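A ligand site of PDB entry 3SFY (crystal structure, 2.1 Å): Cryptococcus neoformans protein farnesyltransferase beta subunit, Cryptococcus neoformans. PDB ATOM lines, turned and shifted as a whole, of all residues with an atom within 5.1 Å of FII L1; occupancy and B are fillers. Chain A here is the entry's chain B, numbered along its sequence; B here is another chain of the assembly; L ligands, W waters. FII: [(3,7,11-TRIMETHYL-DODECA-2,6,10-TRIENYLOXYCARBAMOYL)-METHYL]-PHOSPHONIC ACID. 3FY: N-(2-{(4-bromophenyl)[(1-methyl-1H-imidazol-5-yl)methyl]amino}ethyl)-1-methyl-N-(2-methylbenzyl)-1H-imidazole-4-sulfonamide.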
ATOM      1  N   TRP A  90     -12.388  -3.530  20.441  1.00  0.00           N
ATOM      2  CA  TRP A  90     -13.632  -4.183  20.862  1.00  0.00           C
ATOM      3  C   TRP A  90     -14.395  -3.302  21.832  1.00  0.00           C
ATOM      4  O   TRP A  90     -15.622  -3.151  21.725  1.00  0.00           O
ATOM      5  CB  TRP A  90     -13.381  -5.573  21.474  1.00  0.00           C
ATOM      6  CG  TRP A  90     -13.039  -6.573  20.448  1.00  0.00           C
ATOM      7  CD1 TRP A  90     -11.807  -7.123  20.222  1.00  0.00           C
ATOM      8  CD2 TRP A  90     -13.922  -7.110  19.461  1.00  0.00           C
ATOM      9  NE1 TRP A  90     -11.879  -7.998  19.140  1.00  0.00           N
ATOM     10  CE2 TRP A  90     -13.160  -7.996  18.651  1.00  0.00           C
ATOM     11  CE3 TRP A  90     -15.284  -6.938  19.159  1.00  0.00           C
ATOM     12  CZ2 TRP A  90     -13.708  -8.715  17.587  1.00  0.00           C
ATOM     13  CZ3 TRP A  90     -15.830  -7.643  18.096  1.00  0.00           C
ATOM     14  CH2 TRP A  90     -15.051  -8.519  17.317  1.00  0.00           C
ATOM     15  N   LEU A 141      -9.020  -9.738  14.517  1.00  0.00           N
ATOM     16  CA  LEU A 141     -10.214  -9.445  15.303  1.00  0.00           C
ATOM     17  C   LEU A 141     -10.373  -7.942  15.570  1.00  0.00           C
ATOM     18  O   LEU A 141     -11.421  -7.386  15.259  1.00  0.00           O
ATOM     19  CB  LEU A 141     -10.289 -10.297  16.582  1.00  0.00           C
ATOM     20  CG  LEU A 141     -10.954 -11.681  16.392  1.00  0.00           C
ATOM     21  CD1 LEU A 141     -10.293 -12.520  15.258  1.00  0.00           C
ATOM     22  CD2 LEU A 141     -10.951 -12.458  17.735  1.00  0.00           C
ATOM     23  N   ARG A 197     -13.164 -17.438  13.773  1.00  0.00           N
ATOM     24  CA  ARG A 197     -13.331 -16.030  14.173  1.00  0.00           C
ATOM     25  C   ARG A 197     -12.471 -15.157  13.241  1.00  0.00           C
ATOM     26  O   ARG A 197     -12.914 -14.103  12.809  1.00  0.00           O
ATOM     27  CB  ARG A 197     -12.881 -15.764  15.635  1.00  0.00           C
ATOM     28  CG  ARG A 197     -13.676 -16.412  16.784  1.00  0.00           C
ATOM     29  CD  ARG A 197     -12.818 -16.341  18.116  1.00  0.00           C
ATOM     30  NE  ARG A 197     -11.414 -16.667  17.801  1.00  0.00           N
ATOM     31  CZ  ARG A 197     -10.337 -16.160  18.429  1.00  0.00           C
ATOM     32  NH1 ARG A 197     -10.454 -15.331  19.453  1.00  0.00           N
ATOM     33  NH2 ARG A 197      -9.112 -16.509  18.018  1.00  0.00           N
ATOM     34  N   TYR A 200     -14.013 -15.053   9.838  1.00  0.00           N
ATOM     35  CA  TYR A 200     -15.189 -14.200   9.836  1.00  0.00           C
ATOM     36  C   TYR A 200     -14.775 -12.738   9.769  1.00  0.00           C
ATOM     37  O   TYR A 200     -15.299 -11.965   8.946  1.00  0.00           O
ATOM     38  CB  TYR A 200     -16.079 -14.453  11.070  1.00  0.00           C
ATOM     39  CG  TYR A 200     -17.059 -13.318  11.305  1.00  0.00           C
ATOM     40  CD1 TYR A 200     -18.191 -13.170  10.481  1.00  0.00           C
ATOM     41  CD2 TYR A 200     -16.832 -12.382  12.316  1.00  0.00           C
ATOM     42  CE1 TYR A 200     -19.096 -12.103  10.708  1.00  0.00           C
ATOM     43  CE2 TYR A 200     -17.717 -11.324  12.532  1.00  0.00           C
ATOM     44  CZ  TYR A 200     -18.842 -11.187  11.738  1.00  0.00           C
ATOM     45  OH  TYR A 200     -19.683 -10.123  11.972  1.00  0.00           O
ATOM     46  N   CYS A 201     -13.849 -12.356  10.642  1.00  0.00           N
ATOM     47  CA  CYS A 201     -13.448 -10.948  10.763  1.00  0.00           C
ATOM     48  C   CYS A 201     -12.769 -10.460   9.485  1.00  0.00           C
ATOM     49  O   CYS A 201     -12.988  -9.339   9.041  1.00  0.00           O
ATOM     50  CB  CYS A 201     -12.508 -10.766  11.961  1.00  0.00           C
ATOM     51  SG  CYS A 201     -13.368 -10.870  13.537  1.00  0.00           S
ATOM     52  N   HIS A 266     -20.248 -24.645  18.858  1.00  0.00           N
ATOM     53  CA  HIS A 266     -20.369 -23.536  19.805  1.00  0.00           C
ATOM     54  C   HIS A 266     -21.033 -22.343  19.111  1.00  0.00           C
ATOM     55  O   HIS A 266     -20.749 -22.046  17.941  1.00  0.00           O
ATOM     56  CB  HIS A 266     -19.001 -23.119  20.365  1.00  0.00           C
ATOM     57  CG  HIS A 266     -19.111 -22.186  21.528  1.00  0.00           C
ATOM     58  ND1 HIS A 266     -19.056 -22.609  22.838  1.00  0.00           N
ATOM     59  CD2 HIS A 266     -19.362 -20.854  21.574  1.00  0.00           C
ATOM     60  CE1 HIS A 266     -19.240 -21.581  23.639  1.00  0.00           C
ATOM     61  NE2 HIS A 266     -19.435 -20.498  22.900  1.00  0.00           N
ATOM     62  N   GLY A 268     -20.527 -19.145  19.342  1.00  0.00           N
ATOM     63  CA  GLY A 268     -19.566 -18.155  18.828  1.00  0.00           C
ATOM     64  C   GLY A 268     -19.000 -18.555  17.482  1.00  0.00           C
ATOM     65  O   GLY A 268     -18.951 -17.745  16.542  1.00  0.00           O
ATOM     66  N   TYR A 269     -18.546 -19.806  17.375  1.00  0.00           N
ATOM     67  CA  TYR A 269     -17.946 -20.306  16.150  1.00  0.00           C
ATOM     68  C   TYR A 269     -18.973 -20.628  15.075  1.00  0.00           C
ATOM     69  O   TYR A 269     -18.665 -20.549  13.876  1.00  0.00           O
ATOM     70  CB  TYR A 269     -17.068 -21.525  16.464  1.00  0.00           C
ATOM     71  CG  TYR A 269     -15.941 -21.165  17.419  1.00  0.00           C
ATOM     72  CD1 TYR A 269     -15.045 -20.145  17.110  1.00  0.00           C
ATOM     73  CD2 TYR A 269     -15.774 -21.855  18.613  1.00  0.00           C
ATOM     74  CE1 TYR A 269     -14.011 -19.808  17.986  1.00  0.00           C
ATOM     75  CE2 TYR A 269     -14.739 -21.519  19.498  1.00  0.00           C
ATOM     76  CZ  TYR A 269     -13.868 -20.515  19.169  1.00  0.00           C
ATOM     77  OH  TYR A 269     -12.860 -20.210  20.043  1.00  0.00           O
ATOM     78  N   CYS A 272     -19.750 -17.279  13.504  1.00  0.00           N
ATOM     79  CA  CYS A 272     -18.658 -16.925  12.603  1.00  0.00           C
ATOM     80  C   CYS A 272     -18.614 -17.783  11.348  1.00  0.00           C
ATOM     81  O   CYS A 272     -18.294 -17.268  10.254  1.00  0.00           O
ATOM     82  CB  CYS A 272     -17.319 -16.997  13.335  1.00  0.00           C
ATOM     83  SG  CYS A 272     -17.146 -15.675  14.570  1.00  0.00           S
ATOM     84  N   GLY A 316     -24.720 -21.532  24.590  1.00  0.00           N
ATOM     85  CA  GLY A 316     -23.719 -21.537  23.502  1.00  0.00           C
ATOM     86  C   GLY A 316     -23.325 -22.929  23.015  1.00  0.00           C
ATOM     87  O   GLY A 316     -22.722 -23.068  21.940  1.00  0.00           O
ATOM     88  N   ARG A 317     -23.651 -23.964  23.786  1.00  0.00           N
ATOM     89  CA  ARG A 317     -23.379 -25.346  23.404  1.00  0.00           C
ATOM     90  C   ARG A 317     -24.212 -26.269  24.291  1.00  0.00           C
ATOM     91  O   ARG A 317     -24.658 -25.889  25.370  1.00  0.00           O
ATOM     92  CB  ARG A 317     -21.872 -25.723  23.473  1.00  0.00           C
ATOM     93  CG  ARG A 317     -21.112 -25.161  24.668  1.00  0.00           C
ATOM     94  CD  ARG A 317     -19.637 -25.612  24.722  1.00  0.00           C
ATOM     95  NE  ARG A 317     -18.897 -24.761  25.650  1.00  0.00           N
ATOM     96  CZ  ARG A 317     -17.777 -25.121  26.266  1.00  0.00           C
ATOM     97  NH1 ARG A 317     -17.251 -26.333  26.060  1.00  0.00           N
ATOM     98  NH2 ARG A 317     -17.200 -24.283  27.107  1.00  0.00           N
ATOM     99  N   LYS A 320     -24.574 -26.886  28.419  1.00  0.00           N
ATOM    100  CA  LYS A 320     -24.042 -25.765  29.224  1.00  0.00           C
ATOM    101  C   LYS A 320     -25.165 -24.774  29.473  1.00  0.00           C
ATOM    102  O   LYS A 320     -26.313 -25.114  29.253  1.00  0.00           O
ATOM    103  CB  LYS A 320     -22.863 -25.081  28.537  1.00  0.00           C
ATOM    104  CG  LYS A 320     -21.701 -26.039  28.250  1.00  0.00           C
ATOM    105  CD  LYS A 320     -20.672 -25.940  29.328  1.00  0.00           C
ATOM    106  CE  LYS A 320     -19.722 -24.860  29.072  1.00  0.00           C
ATOM    107  NZ  LYS A 320     -19.209 -24.302  30.345  1.00  0.00           N
ATOM    108  N   LEU A 321     -24.837 -23.567  29.920  1.00  0.00           N
ATOM    109  CA  LEU A 321     -25.832 -22.625  30.462  1.00  0.00           C
ATOM    110  C   LEU A 321     -26.202 -21.500  29.511  1.00  0.00           C
ATOM    111  O   LEU A 321     -25.368 -21.035  28.707  1.00  0.00           O
ATOM    112  CB  LEU A 321     -25.317 -22.021  31.778  1.00  0.00           C
ATOM    113  CG  LEU A 321     -24.815 -22.976  32.869  1.00  0.00           C
ATOM    114  CD1 LEU A 321     -24.083 -22.189  33.982  1.00  0.00           C
ATOM    115  CD2 LEU A 321     -25.965 -23.814  33.452  1.00  0.00           C
ATOM    116  N   ASP A 323     -26.997 -17.752  28.295  1.00  0.00           N
ATOM    117  CA  ASP A 323     -26.164 -16.580  28.482  1.00  0.00           C
ATOM    118  C   ASP A 323     -26.610 -15.517  27.468  1.00  0.00           C
ATOM    119  O   ASP A 323     -26.713 -15.791  26.265  1.00  0.00           O
ATOM    120  CB  ASP A 323     -24.684 -16.978  28.320  1.00  0.00           C
ATOM    121  CG  ASP A 323     -23.723 -15.787  28.273  1.00  0.00           C
ATOM    122  OD1 ASP A 323     -24.159 -14.616  28.081  1.00  0.00           O
ATOM    123  OD2 ASP A 323     -22.495 -16.039  28.392  1.00  0.00           O
ATOM    124  N   TYR A 326     -25.285 -14.909  23.789  1.00  0.00           N
ATOM    125  CA  TYR A 326     -25.687 -15.842  22.713  1.00  0.00           C
ATOM    126  C   TYR A 326     -26.952 -15.417  21.997  1.00  0.00           C
ATOM    127  O   TYR A 326     -27.278 -15.948  20.951  1.00  0.00           O
ATOM    128  CB  TYR A 326     -25.791 -17.288  23.252  1.00  0.00           C
ATOM    129  CG  TYR A 326     -24.446 -17.780  23.750  1.00  0.00           C
ATOM    130  CD1 TYR A 326     -23.321 -17.709  22.925  1.00  0.00           C
ATOM    131  CD2 TYR A 326     -24.297 -18.281  25.039  1.00  0.00           C
ATOM    132  CE1 TYR A 326     -22.051 -18.116  23.381  1.00  0.00           C
ATOM    133  CE2 TYR A 326     -23.047 -18.728  25.503  1.00  0.00           C
ATOM    134  CZ  TYR A 326     -21.929 -18.613  24.682  1.00  0.00           C
ATOM    135  OH  TYR A 326     -20.694 -19.055  25.117  1.00  0.00           O
ATOM    136  N   TRP A 329     -24.876 -14.308  19.196  1.00  0.00           N
ATOM    137  CA  TRP A 329     -24.095 -15.341  18.484  1.00  0.00           C
ATOM    138  C   TRP A 329     -24.997 -16.422  17.905  1.00  0.00           C
ATOM    139  O   TRP A 329     -24.812 -16.851  16.760  1.00  0.00           O
ATOM    140  CB  TRP A 329     -23.002 -15.959  19.351  1.00  0.00           C
ATOM    141  CG  TRP A 329     -22.060 -14.930  19.875  1.00  0.00           C
ATOM    142  CD1 TRP A 329     -21.858 -14.593  21.180  1.00  0.00           C
ATOM    143  CD2 TRP A 329     -21.243 -14.055  19.095  1.00  0.00           C
ATOM    144  NE1 TRP A 329     -20.945 -13.577  21.272  1.00  0.00           N
ATOM    145  CE2 TRP A 329     -20.550 -13.225  20.002  1.00  0.00           C
ATOM    146  CE3 TRP A 329     -21.011 -13.900  17.724  1.00  0.00           C
ATOM    147  CZ2 TRP A 329     -19.624 -12.257  19.577  1.00  0.00           C
ATOM    148  CZ3 TRP A 329     -20.098 -12.916  17.291  1.00  0.00           C
ATOM    149  CH2 TRP A 329     -19.427 -12.106  18.228  1.00  0.00           C
ATOM    150  N   TYR A 409     -19.193  -5.927  26.519  1.00  0.00           N
ATOM    151  CA  TYR A 409     -19.400  -7.047  25.622  1.00  0.00           C
ATOM    152  C   TYR A 409     -20.835  -7.633  25.713  1.00  0.00           C
ATOM    153  O   TYR A 409     -21.489  -7.872  24.692  1.00  0.00           O
ATOM    154  CB  TYR A 409     -18.343  -8.119  25.922  1.00  0.00           C
ATOM    155  CG  TYR A 409     -18.664  -9.483  25.341  1.00  0.00           C
ATOM    156  CD1 TYR A 409     -18.224  -9.831  24.043  1.00  0.00           C
ATOM    157  CD2 TYR A 409     -19.379 -10.426  26.071  1.00  0.00           C
ATOM    158  CE1 TYR A 409     -18.506 -11.081  23.500  1.00  0.00           C
ATOM    159  CE2 TYR A 409     -19.677 -11.688  25.528  1.00  0.00           C
ATOM    160  CZ  TYR A 409     -19.232 -12.011  24.252  1.00  0.00           C
ATOM    161  OH  TYR A 409     -19.530 -13.238  23.731  1.00  0.00           O
ATOM    162  N   TYR B 122      -6.648 -17.581  25.347  1.00  0.00           N
ATOM    163  CA  TYR B 122      -6.368 -17.962  23.942  1.00  0.00           C
ATOM    164  C   TYR B 122      -4.853 -18.103  23.729  1.00  0.00           C
ATOM    165  O   TYR B 122      -4.406 -18.881  22.878  1.00  0.00           O
ATOM    166  CB  TYR B 122      -6.891 -16.930  22.919  1.00  0.00           C
ATOM    167  CG  TYR B 122      -8.280 -17.201  22.371  1.00  0.00           C
ATOM    168  CD1 TYR B 122      -8.499 -18.184  21.396  1.00  0.00           C
ATOM    169  CD2 TYR B 122      -9.381 -16.466  22.819  1.00  0.00           C
ATOM    170  CE1 TYR B 122      -9.776 -18.440  20.896  1.00  0.00           C
ATOM    171  CE2 TYR B 122     -10.670 -16.707  22.331  1.00  0.00           C
ATOM    172  CZ  TYR B 122     -10.860 -17.695  21.374  1.00  0.00           C
ATOM    173  OH  TYR B 122     -12.133 -17.925  20.886  1.00  0.00           O
ATOM    174  N   TYR B 158     -13.211 -25.210  26.728  1.00  0.00           N
ATOM    175  CA  TYR B 158     -13.291 -25.355  25.293  1.00  0.00           C
ATOM    176  C   TYR B 158     -11.914 -25.412  24.610  1.00  0.00           C
ATOM    177  O   TYR B 158     -11.665 -26.274  23.759  1.00  0.00           O
ATOM    178  CB  TYR B 158     -14.151 -24.251  24.658  1.00  0.00           C
ATOM    179  CG  TYR B 158     -14.480 -24.529  23.202  1.00  0.00           C
ATOM    180  CD1 TYR B 158     -15.708 -25.075  22.837  1.00  0.00           C
ATOM    181  CD2 TYR B 158     -13.551 -24.269  22.177  1.00  0.00           C
ATOM    182  CE1 TYR B 158     -16.032 -25.347  21.491  1.00  0.00           C
ATOM    183  CE2 TYR B 158     -13.852 -24.537  20.831  1.00  0.00           C
ATOM    184  CZ  TYR B 158     -15.099 -25.077  20.508  1.00  0.00           C
ATOM    185  OH  TYR B 158     -15.413 -25.346  19.192  1.00  0.00           O
ATOM    186  N   HIS B 159     -11.029 -24.483  24.977  1.00  0.00           N
ATOM    187  CA  HIS B 159      -9.718 -24.419  24.346  1.00  0.00           C
ATOM    188  C   HIS B 159      -8.860 -25.645  24.700  1.00  0.00           C
ATOM    189  O   HIS B 159      -8.012 -26.058  23.915  1.00  0.00           O
ATOM    190  CB  HIS B 159      -8.980 -23.124  24.707  1.00  0.00           C
ATOM    191  CG  HIS B 159      -9.757 -21.890  24.361  1.00  0.00           C
ATOM    192  ND1 HIS B 159     -10.657 -21.847  23.320  1.00  0.00           N
ATOM    193  CD2 HIS B 159      -9.763 -20.655  24.922  1.00  0.00           C
ATOM    194  CE1 HIS B 159     -11.205 -20.647  23.255  1.00  0.00           C
ATOM    195  NE2 HIS B 159     -10.672 -19.905  24.220  1.00  0.00           N
HETATM  196  C1  FII L   1     -14.346 -12.313  17.509  1.00  0.00           C
HETATM  197  C2  FII L   1     -15.517 -13.289  17.590  1.00  0.00           C
HETATM  198  C6  FII L   1     -16.674 -13.168  16.604  1.00  0.00           C
HETATM  199  C10 FII L   1     -15.533 -14.278  18.564  1.00  0.00           C
HETATM  200  C11 FII L   1     -16.531 -15.224  18.752  1.00  0.00           C
HETATM  201  C12 FII L   1     -17.378 -14.895  19.982  1.00  0.00           C
HETATM  202  C15 FII L   1     -17.503 -16.121  20.901  1.00  0.00           C
HETATM  203  C18 FII L   1     -18.683 -16.224  21.875  1.00  0.00           C
HETATM  204  C22 FII L   1     -16.555 -17.136  20.837  1.00  0.00           C
HETATM  205  C23 FII L   1     -16.555 -18.291  21.607  1.00  0.00           C
HETATM  206  C24 FII L   1     -15.233 -18.442  22.373  1.00  0.00           C
HETATM  207  C27 FII L   1     -15.256 -19.689  23.257  1.00  0.00           C
HETATM  208  C30 FII L   1     -15.784 -21.009  22.717  1.00  0.00           C
HETATM  209  C34 FII L   1     -14.790 -19.608  24.573  1.00  0.00           C
HETATM  210  C35 FII L   1     -14.753 -20.651  25.482  1.00  0.00           C
HETATM  211  O36 FII L   1     -14.881 -20.137  26.812  1.00  0.00           O
HETATM  212  N42 FII L   1     -16.163 -19.721  27.009  1.00  0.00           N
HETATM  213  C43 FII L   1     -17.013 -20.496  27.678  1.00  0.00           C
HETATM  214  O44 FII L   1     -16.717 -21.588  28.152  1.00  0.00           O
HETATM  215  C45 FII L   1     -18.424 -19.921  27.832  1.00  0.00           C
HETATM  216  P46 FII L   1     -19.684 -21.183  27.511  1.00  0.00           P
HETATM  217  O49 FII L   1     -19.035 -22.157  26.387  1.00  0.00           O
HETATM  218  O50 FII L   1     -19.756 -22.077  28.857  1.00  0.00           O
HETATM  219  O51 FII L   1     -20.994 -20.624  27.108  1.00  0.00           O
HETATM  220  CAA 3FY L   2     -14.320 -11.083  21.291  1.00  0.00           C
HETATM  221  CAB 3FY L   2      -9.851 -17.658  26.904  1.00  0.00           C
HETATM  222  CAC 3FY L   2     -17.436 -16.452  30.056  1.00  0.00           C
HETATM  223  OAD 3FY L   2     -15.355 -15.992  24.453  1.00  0.00           O
HETATM  224  OAE 3FY L   2     -13.464 -15.806  22.949  1.00  0.00           O
HETATM  225 BRAF 3FY L   2     -16.075  -6.912  28.734  1.00  0.00          BR
HETATM  226  CAG 3FY L   2     -11.886  -9.446  23.691  1.00  0.00           C
HETATM  227  CAH 3FY L   2     -11.672 -10.459  24.616  1.00  0.00           C
HETATM  228  CAI 3FY L   2     -12.739  -9.650  22.599  1.00  0.00           C
HETATM  229  CAJ 3FY L   2     -15.175  -9.315  27.405  1.00  0.00           C
HETATM  230  CAK 3FY L   2     -16.617  -9.718  29.278  1.00  0.00           C
HETATM  231  CAL 3FY L   2     -12.319 -11.683  24.458  1.00  0.00           C
HETATM  232  CAM 3FY L   2     -15.066 -10.685  27.191  1.00  0.00           C
HETATM  233  CAN 3FY L   2     -16.524 -11.100  29.063  1.00  0.00           C
HETATM  234  CAO 3FY L   2     -18.527 -13.931  27.747  1.00  0.00           C
HETATM  235  CAP 3FY L   2     -19.385 -15.666  28.690  1.00  0.00           C
HETATM  236  CAQ 3FY L   2     -12.338 -17.502  27.271  1.00  0.00           C
HETATM  237  CAR 3FY L   2     -11.603 -16.529  25.458  1.00  0.00           C
HETATM  238  CAS 3FY L   2     -14.635 -13.514  26.847  1.00  0.00           C
HETATM  239  CAT 3FY L   2     -15.073 -13.458  25.381  1.00  0.00           C
HETATM  240  CAU 3FY L   2     -13.865 -13.252  23.269  1.00  0.00           C
HETATM  241  CAV 3FY L   2     -16.152 -13.952  28.750  1.00  0.00           C
HETATM  242  NAW 3FY L   2     -19.626 -14.670  27.865  1.00  0.00           N
HETATM  243  NAX 3FY L   2     -13.389 -16.965  26.637  1.00  0.00           N
HETATM  244  CAY 3FY L   2     -13.385 -10.876  22.461  1.00  0.00           C
HETATM  245  CAZ 3FY L   2     -15.939  -8.805  28.456  1.00  0.00           C
HETATM  246  CBA 3FY L   2     -15.740 -11.619  28.001  1.00  0.00           C
HETATM  247  CBB 3FY L   2     -13.179 -11.894  23.376  1.00  0.00           C
HETATM  248  CBC 3FY L   2     -17.581 -14.449  28.517  1.00  0.00           C
HETATM  249  CBD 3FY L   2     -12.923 -16.378  25.534  1.00  0.00           C
HETATM  250  NBE 3FY L   2     -15.610 -12.950  27.799  1.00  0.00           N
HETATM  251  NBF 3FY L   2     -13.902 -13.906  24.593  1.00  0.00           N
HETATM  252  NBG 3FY L   2     -11.259 -17.237  26.534  1.00  0.00           N
HETATM  253  NBH 3FY L   2     -18.128 -15.515  29.101  1.00  0.00           N
HETATM  254  SBI 3FY L   2     -13.943 -15.509  24.344  1.00  0.00           S
HETATM  255  O   HOH W   1     -18.527 -21.024  31.049  1.00  0.00           O
HETATM  256  O   HOH W   2     -14.568 -23.031  28.033  1.00  0.00           O
HETATM  257  O   HOH W   3     -21.448 -18.353  28.913  1.00  0.00           O
HETATM  258  O   HOH W   4     -22.018 -22.094  30.296  1.00  0.00           O
HETATM  259  O   HOH W   5     -16.593 -17.154  26.177  1.00  0.00           O
HETATM  260  O   HOH W   6     -23.366 -21.970  26.999  1.00  0.00           O
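Water W2 lies within hydrogen-bond range of O44 of FII L1, N of Tyr 158 of chain B and NH2 of Arg 317. Water W4 lies within hydrogen-bond range of an oxygen (O50) of FII L1 and the backbone NH (N) of Leu 321. Water W1 bridges O50 of FII L1 (2.7 Å) and NZ of Lys 320 (3.4 Å). Water W6 lies within hydrogen-bond range of O51 of FII L1 (2.7 Å), O of Leu 321 (2.8 Å) and N of Gly 316 (2.8 Å). Water W5 lies within hydrogen-bond range of an oxygen (OAD) of 3FY L2 (2.4 Å) and a nitrogen (N42) of FII L1 (2.7 Å).
Residues that only touch FII L1: Trp 90, Leu 141, Arg 197, His 266, Gly 268, Tyr 269, Cys 272, Trp 329, Tyr 409, Tyr 122 of chain B, Tyr 158 of chain B and His 159 of chain B. Hydrophobic or aromatic side chains within 4 Å of FII L1: Trp 90, Leu 141, His 266, Tyr 269, Tyr 326, Trp 329, Tyr 158 of chain B and His 159 of chain B. Of the 20 residues printed, 15 come within 4 Å of FII L1.
The side-chain hydroxyl (OH) of Tyr 326 lies within hydrogen-bond range of a ring nitrogen (NE2) of His 266, at 2.9 Å. SG of Cys 272 sits at hydrogen-bond distance from O of Gly 268 (3.4 Å). The guanidinium group (NH1) of Arg 197 sits close to the side-chain hydroxyl (OH) of Tyr 122 of chain B, 3.4 Å away. The backbone carbonyl oxygen (O) of Arg 197 is in hydrogen-bond range of the side-chain sulfur (SG) of Cys 201 (3.3 Å). OH of Tyr 409 sits at hydrogen-bond distance from NE1 of Trp 329, 2.9 Å away. The side-chain hydroxyl of Tyr 122 of chain B sits at hydrogen-bond distance from the side-chain hydroxyl of Tyr 269 (2.5 Å).
An oxygen (O51) of FII L1 is in hydrogen-bond range of the side-chain hydroxyl of Tyr 326. The guanidinium group of Arg 317 is in salt-bridge range of an oxygen (O49) of FII L1, 2.7 Å away. The side-chain amino group (NZ) of Lys 320 is in salt-bridge range of an oxygen (O50) of FII L1 (2.7 Å). The side-chain hydroxyl (OH) of Tyr 122 of chain B sits close to an oxygen (OAE) of 3FY L2 (3.2 Å).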
